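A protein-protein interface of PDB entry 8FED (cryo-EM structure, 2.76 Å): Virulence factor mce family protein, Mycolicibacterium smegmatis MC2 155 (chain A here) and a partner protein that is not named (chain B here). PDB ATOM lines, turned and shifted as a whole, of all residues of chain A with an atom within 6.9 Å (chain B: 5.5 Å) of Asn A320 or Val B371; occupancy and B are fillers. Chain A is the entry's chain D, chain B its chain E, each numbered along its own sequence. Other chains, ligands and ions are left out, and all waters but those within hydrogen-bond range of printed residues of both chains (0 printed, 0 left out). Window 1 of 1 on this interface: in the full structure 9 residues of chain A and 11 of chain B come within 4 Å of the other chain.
O of Asn A320 sits close to OD1 of Asn B341. The side-chain amide nitrogen (NE2) of Gln A321 lies within hydrogen-bond range of the backbone carbonyl oxygen (O) of Asn B341 (3.1 Å). NZ of Lys A393 is in hydrogen-bond range of O of Val B371 (2.5 Å).
The side-chain amide nitrogen (ND2) of Asn A320 sits at hydrogen-bond distance from the backbone carbonyl oxygen (O) of Ala A388 (3.0 Å). ND2 of Asn A320 is in hydrogen-bond range of O of Met A389 (3.1 Å). O of Thr A390 lies within hydrogen-bond range of ND2 of Asn A320. The side-chain amide oxygen (OD1) of Asn A320 lies within hydrogen-bond range of the side-chain amide nitrogen (NE2) of Gln A394, at 2.6 Å. O of Ala A388 lies within hydrogen-bond range of NE2 of Gln A321. NH2 of Arg B372 sits at hydrogen-bond distance from O of Ser B350 (2.7 Å).
Among the printed residues, merely in contact across the chains: Ala A388 with Ser B345 (3.3 Å), Asn A320 with Val B371 (3.5 Å), Lys A393 with Arg B372 (3.7 Å) and Gln A321 with Ile B368 (3.9 Å).
Asn A317 touches none of the printed residues of chain B. Of chain B, only Asn B341 (3.2 Å) and Val B371 (3.5 Å) come within 4 Å of Asn A320. Printed residues of chain B within 4 Å of Ala A388: Ser B345 (3.3 Å). Of the printed residues of chain A, Asn B341 touches Asn A320 (3.2 Å) and Gln A321 (3.1 Å). Of the printed residues of chain A, Ser B345 touches Ala A388. Of the printed residues of chain A, Ile B368 touches Gln A321. Val B371 touches just these residues of chain A: Asn A320 and Lys A393. Printed residues of chain A within 4 Å of Arg B372: Lys A393. The nearest residue of chain B that does not touch Asn A320 is Ser B345 (4.8 Å).
Printed residues of chain A that touch a printed residue of chain B: Asn A320, Gln A321, Ala A388 and Lys A393. Hydrophobic or aromatic side chains of chain A within 4 Å of the printed part of chain B: Ala A388. Along chain A the printed residues that touch a printed residue of chain B span positions 320 to 393. Of the 10 printed residues of chain B, 5 touch a printed residue of chain A. Hydrophobic or aromatic side chains of chain B within 4 Å of the printed part of chain A: Ile B368 and Val B371. Among the printed residues, no Asp or Glu carboxylate lies within 4 Å of a Lys or Arg side-chain nitrogen of the other chain.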
ATOM      1  N   ASN A 317     -32.735 -10.072   5.230  1.00  0.00           N
ATOM      2  CA  ASN A 317     -31.384 -10.509   4.905  1.00  0.00           C
ATOM      3  C   ASN A 317     -30.354  -9.455   5.287  1.00  0.00           C
ATOM      4  O   ASN A 317     -30.531  -8.267   5.007  1.00  0.00           O
ATOM      5  CB  ASN A 317     -31.283 -10.822   3.417  1.00  0.00           C
ATOM      6  CG  ASN A 317     -32.439 -11.657   2.924  1.00  0.00           C
ATOM      7  OD1 ASN A 317     -32.559 -12.834   3.265  1.00  0.00           O
ATOM      8  ND2 ASN A 317     -33.295 -11.059   2.110  1.00  0.00           N
ATOM      9  N   SER A 318     -29.269  -9.899   5.920  1.00  0.00           N
ATOM     10  CA  SER A 318     -28.175  -9.014   6.282  1.00  0.00           C
ATOM     11  C   SER A 318     -27.019  -9.247   5.325  1.00  0.00           C
ATOM     12  O   SER A 318     -26.401 -10.320   5.371  1.00  0.00           O
ATOM     13  CB  SER A 318     -27.734  -9.262   7.722  1.00  0.00           C
ATOM     14  OG  SER A 318     -27.503 -10.639   7.951  1.00  0.00           O
ATOM     15  N   PRO A 319     -26.712  -8.303   4.431  1.00  0.00           N
ATOM     16  CA  PRO A 319     -25.643  -8.545   3.446  1.00  0.00           C
ATOM     17  C   PRO A 319     -24.286  -8.853   4.054  1.00  0.00           C
ATOM     18  O   PRO A 319     -23.564  -9.709   3.530  1.00  0.00           O
ATOM     19  CB  PRO A 319     -25.620  -7.238   2.644  1.00  0.00           C
ATOM     20  CG  PRO A 319     -26.996  -6.690   2.783  1.00  0.00           C
ATOM     21  CD  PRO A 319     -27.431  -7.047   4.173  1.00  0.00           C
ATOM     22  N   ASN A 320     -23.915  -8.187   5.149  1.00  0.00           N
ATOM     23  CA  ASN A 320     -22.578  -8.369   5.704  1.00  0.00           C
ATOM     24  C   ASN A 320     -22.437  -9.693   6.445  1.00  0.00           C
ATOM     25  O   ASN A 320     -21.387 -10.339   6.366  1.00  0.00           O
ATOM     26  CB  ASN A 320     -22.232  -7.208   6.634  1.00  0.00           C
ATOM     27  CG  ASN A 320     -21.984  -5.922   5.886  1.00  0.00           C
ATOM     28  OD1 ASN A 320     -21.633  -5.938   4.707  1.00  0.00           O
ATOM     29  ND2 ASN A 320     -22.168  -4.799   6.564  1.00  0.00           N
ATOM     30  N   GLN A 321     -23.463 -10.106   7.179  1.00  0.00           N
ATOM     31  CA  GLN A 321     -23.397 -11.353   7.925  1.00  0.00           C
ATOM     32  C   GLN A 321     -23.940 -12.546   7.152  1.00  0.00           C
ATOM     33  O   GLN A 321     -23.752 -13.684   7.591  1.00  0.00           O
ATOM     34  CB  GLN A 321     -24.157 -11.222   9.252  1.00  0.00           C
ATOM     35  CG  GLN A 321     -23.560 -10.225  10.241  1.00  0.00           C
ATOM     36  CD  GLN A 321     -23.871  -8.777   9.901  1.00  0.00           C
ATOM     37  OE1 GLN A 321     -24.889  -8.478   9.278  1.00  0.00           O
ATOM     38  NE2 GLN A 321     -22.992  -7.871  10.312  1.00  0.00           N
ATOM     39  N   GLY A 322     -24.603 -12.318   6.019  1.00  0.00           N
ATOM     40  CA  GLY A 322     -25.149 -13.398   5.219  1.00  0.00           C
ATOM     41  C   GLY A 322     -26.336 -14.104   5.843  1.00  0.00           C
ATOM     42  O   GLY A 322     -26.523 -14.069   7.061  1.00  0.00           O
ATOM     43  N   ALA A 388     -23.769  -3.577  12.186  1.00  0.00           N
ATOM     44  CA  ALA A 388     -23.774  -2.953  10.863  1.00  0.00           C
ATOM     45  C   ALA A 388     -24.206  -3.989   9.833  1.00  0.00           C
ATOM     46  O   ALA A 388     -23.400  -4.772   9.331  1.00  0.00           O
ATOM     47  CB  ALA A 388     -22.403  -2.380  10.532  1.00  0.00           C
ATOM     48  N   MET A 389     -25.504  -3.994   9.518  1.00  0.00           N
ATOM     49  CA  MET A 389     -26.033  -4.963   8.563  1.00  0.00           C
ATOM     50  C   MET A 389     -25.484  -4.727   7.161  1.00  0.00           C
ATOM     51  O   MET A 389     -25.106  -5.679   6.470  1.00  0.00           O
ATOM     52  CB  MET A 389     -27.559  -4.916   8.552  1.00  0.00           C
ATOM     53  CG  MET A 389     -28.209  -5.476   9.804  1.00  0.00           C
ATOM     54  SD  MET A 389     -29.994  -5.645   9.631  1.00  0.00           S
ATOM     55  CE  MET A 389     -30.412  -6.412  11.193  1.00  0.00           C
ATOM     56  N   THR A 390     -25.439  -3.477   6.719  1.00  0.00           N
ATOM     57  CA  THR A 390     -24.943  -3.131   5.395  1.00  0.00           C
ATOM     58  C   THR A 390     -23.775  -2.158   5.521  1.00  0.00           C
ATOM     59  O   THR A 390     -23.371  -1.771   6.619  1.00  0.00           O
ATOM     60  CB  THR A 390     -26.051  -2.528   4.527  1.00  0.00           C
ATOM     61  OG1 THR A 390     -26.304  -1.181   4.942  1.00  0.00           O
ATOM     62  CG2 THR A 390     -27.329  -3.337   4.651  1.00  0.00           C
ATOM     63  N   LEU A 391     -23.232  -1.770   4.378  1.00  0.00           N
ATOM     64  CA  LEU A 391     -22.138  -0.819   4.274  1.00  0.00           C
ATOM     65  C   LEU A 391     -22.480   0.198   3.198  1.00  0.00           C
ATOM     66  O   LEU A 391     -23.295  -0.080   2.312  1.00  0.00           O
ATOM     67  CB  LEU A 391     -20.820  -1.530   3.933  1.00  0.00           C
ATOM     68  CG  LEU A 391     -20.293  -2.540   4.954  1.00  0.00           C
ATOM     69  CD1 LEU A 391     -18.991  -3.151   4.474  1.00  0.00           C
ATOM     70  CD2 LEU A 391     -20.106  -1.886   6.310  1.00  0.00           C
ATOM     71  N   LYS A 393     -20.938   1.103   0.618  1.00  0.00           N
ATOM     72  CA  LYS A 393     -20.598   0.638  -0.720  1.00  0.00           C
ATOM     73  C   LYS A 393     -21.607  -0.359  -1.275  1.00  0.00           C
ATOM     74  O   LYS A 393     -21.724  -0.483  -2.498  1.00  0.00           O
ATOM     75  CB  LYS A 393     -19.206   0.001  -0.716  1.00  0.00           C
ATOM     76  CG  LYS A 393     -19.093  -1.213   0.189  1.00  0.00           C
ATOM     77  CD  LYS A 393     -17.768  -1.929   0.011  1.00  0.00           C
ATOM     78  CE  LYS A 393     -17.772  -3.256   0.748  1.00  0.00           C
ATOM     79  NZ  LYS A 393     -16.514  -4.021   0.542  1.00  0.00           N
ATOM     80  N   GLN A 394     -22.335  -1.063  -0.412  1.00  0.00           N
ATOM     81  CA  GLN A 394     -23.203  -2.158  -0.822  1.00  0.00           C
ATOM     82  C   GLN A 394     -24.626  -1.717  -1.131  1.00  0.00           C
ATOM     83  O   GLN A 394     -25.483  -2.573  -1.370  1.00  0.00           O
ATOM     84  CB  GLN A 394     -23.236  -3.236   0.261  1.00  0.00           C
ATOM     85  CG  GLN A 394     -21.879  -3.773   0.654  1.00  0.00           C
ATOM     86  CD  GLN A 394     -21.984  -4.928   1.622  1.00  0.00           C
ATOM     87  OE1 GLN A 394     -23.027  -5.568   1.726  1.00  0.00           O
ATOM     88  NE2 GLN A 394     -20.904  -5.199   2.342  1.00  0.00           N
ATOM     89  N   ASN B 341     -17.289 -10.943  11.482  1.00  0.00           N
ATOM     90  CA  ASN B 341     -18.330 -10.539  10.542  1.00  0.00           C
ATOM     91  C   ASN B 341     -19.591 -10.088  11.269  1.00  0.00           C
ATOM     92  O   ASN B 341     -20.247  -9.128  10.847  1.00  0.00           O
ATOM     93  CB  ASN B 341     -18.640 -11.678   9.573  1.00  0.00           C
ATOM     94  CG  ASN B 341     -18.551 -11.244   8.124  1.00  0.00           C
ATOM     95  OD1 ASN B 341     -18.600 -10.053   7.817  1.00  0.00           O
ATOM     96  ND2 ASN B 341     -18.417 -12.210   7.225  1.00  0.00           N
ATOM     97  N   SER B 345     -18.045  -5.616  12.195  1.00  0.00           N
ATOM     98  CA  SER B 345     -18.137  -5.120  10.829  1.00  0.00           C
ATOM     99  C   SER B 345     -18.574  -3.661  10.812  1.00  0.00           C
ATOM    100  O   SER B 345     -19.376  -3.225  11.641  1.00  0.00           O
ATOM    101  CB  SER B 345     -19.116  -5.969  10.020  1.00  0.00           C
ATOM    102  OG  SER B 345     -18.724  -7.330  10.006  1.00  0.00           O
ATOM    103  N   SER B 350     -12.407  -3.490  12.132  1.00  0.00           N
ATOM    104  CA  SER B 350     -12.851  -4.575  11.262  1.00  0.00           C
ATOM    105  C   SER B 350     -11.743  -5.589  11.007  1.00  0.00           C
ATOM    106  O   SER B 350     -12.026  -6.752  10.700  1.00  0.00           O
ATOM    107  CB  SER B 350     -13.366  -4.005   9.941  1.00  0.00           C
ATOM    108  OG  SER B 350     -13.861  -5.032   9.100  1.00  0.00           O
ATOM    109  N   ILE B 368     -15.807 -17.299   5.989  1.00  0.00           N
ATOM    110  CA  ILE B 368     -16.823 -16.430   5.384  1.00  0.00           C
ATOM    111  C   ILE B 368     -16.134 -15.193   4.813  1.00  0.00           C
ATOM    112  O   ILE B 368     -15.178 -14.681   5.431  1.00  0.00           O
ATOM    113  CB  ILE B 368     -17.896 -16.060   6.429  1.00  0.00           C
ATOM    114  CG1 ILE B 368     -18.999 -15.178   5.839  1.00  0.00           C
ATOM    115  CG2 ILE B 368     -17.271 -15.421   7.666  1.00  0.00           C
ATOM    116  CD1 ILE B 368     -20.225 -15.070   6.712  1.00  0.00           C
ATOM    117  N   PRO B 369     -16.515 -14.716   3.623  1.00  0.00           N
ATOM    118  CA  PRO B 369     -15.723 -13.677   2.947  1.00  0.00           C
ATOM    119  C   PRO B 369     -15.563 -12.405   3.767  1.00  0.00           C
ATOM    120  O   PRO B 369     -16.468 -11.988   4.492  1.00  0.00           O
ATOM    121  CB  PRO B 369     -16.516 -13.416   1.665  1.00  0.00           C
ATOM    122  CG  PRO B 369     -17.189 -14.702   1.391  1.00  0.00           C
ATOM    123  CD  PRO B 369     -17.531 -15.291   2.724  1.00  0.00           C
ATOM    124  N   ASP B 370     -14.387 -11.793   3.642  1.00  0.00           N
ATOM    125  CA  ASP B 370     -14.085 -10.530   4.307  1.00  0.00           C
ATOM    126  C   ASP B 370     -14.771  -9.406   3.545  1.00  0.00           C
ATOM    127  O   ASP B 370     -14.322  -9.018   2.463  1.00  0.00           O
ATOM    128  CB  ASP B 370     -12.577 -10.307   4.371  1.00  0.00           C
ATOM    129  CG  ASP B 370     -11.862 -11.384   5.160  1.00  0.00           C
ATOM    130  OD1 ASP B 370     -12.533 -12.336   5.611  1.00  0.00           O
ATOM    131  OD2 ASP B 370     -10.630 -11.278   5.330  1.00  0.00           O
ATOM    132  N   VAL B 371     -15.843  -8.862   4.128  1.00  0.00           N
ATOM    133  CA  VAL B 371     -16.724  -7.933   3.428  1.00  0.00           C
ATOM    134  C   VAL B 371     -16.029  -6.641   3.021  1.00  0.00           C
ATOM    135  O   VAL B 371     -16.538  -5.916   2.162  1.00  0.00           O
ATOM    136  CB  VAL B 371     -17.956  -7.625   4.299  1.00  0.00           C
ATOM    137  CG1 VAL B 371     -18.676  -8.905   4.662  1.00  0.00           C
ATOM    138  CG2 VAL B 371     -17.544  -6.872   5.552  1.00  0.00           C
ATOM    139  N   ARG B 372     -14.879  -6.327   3.615  1.00  0.00           N
ATOM    140  CA  ARG B 372     -14.203  -5.080   3.290  1.00  0.00           C
ATOM    141  C   ARG B 372     -13.318  -5.180   2.055  1.00  0.00           C
ATOM    142  O   ARG B 372     -12.869  -4.143   1.552  1.00  0.00           O
ATOM    143  CB  ARG B 372     -13.369  -4.616   4.488  1.00  0.00           C
ATOM    144  CG  ARG B 372     -11.915  -5.057   4.454  1.00  0.00           C
ATOM    145  CD  ARG B 372     -11.151  -4.559   5.666  1.00  0.00           C
ATOM    146  NE  ARG B 372     -11.415  -5.379   6.841  1.00  0.00           N
ATOM    147  CZ  ARG B 372     -10.703  -6.444   7.180  1.00  0.00           C
ATOM    148  NH1 ARG B 372      -9.665  -6.838   6.461  1.00  0.00           N
ATOM    149  NH2 ARG B 372     -11.041  -7.131   8.266  1.00  0.00           N
ATOM    150  N   PHE B 373     -13.075  -6.384   1.538  1.00  0.00           N
ATOM    151  CA  PHE B 373     -12.181  -6.563   0.401  1.00  0.00           C
ATOM    152  C   PHE B 373     -12.802  -7.299  -0.777  1.00  0.00           C
ATOM    153  O   PHE B 373     -12.464  -6.983  -1.919  1.00  0.00           O
ATOM    154  CB  PHE B 373     -10.910  -7.309   0.835  1.00  0.00           C
ATOM    155  CG  PHE B 373      -9.973  -6.477   1.665  1.00  0.00           C
ATOM    156  CD1 PHE B 373      -9.858  -5.114   1.446  1.00  0.00           C
ATOM    157  CD2 PHE B 373      -9.217  -7.056   2.668  1.00  0.00           C
ATOM    158  CE1 PHE B 373      -9.000  -4.346   2.210  1.00  0.00           C
ATOM    159  CE2 PHE B 373      -8.358  -6.290   3.437  1.00  0.00           C
ATOM    160  CZ  PHE B 373      -8.250  -4.935   3.206  1.00  0.00           C
ATOM    161  N   THR B 374     -13.681  -8.266  -0.541  1.00  0.00           N
ATOM    162  CA  THR B 374     -14.293  -8.997  -1.647  1.00  0.00           C
ATOM    163  C   THR B 374     -15.208  -8.072  -2.447  1.00  0.00           C
ATOM    164  O   THR B 374     -16.035  -7.365  -1.860  1.00  0.00           O
ATOM    165  CB  THR B 374     -15.062 -10.227  -1.142  1.00  0.00           C
ATOM    166  OG1 THR B 374     -15.760 -10.839  -2.233  1.00  0.00           O
ATOM    167  CG2 THR B 374     -16.056  -9.873  -0.050  1.00  0.00           C
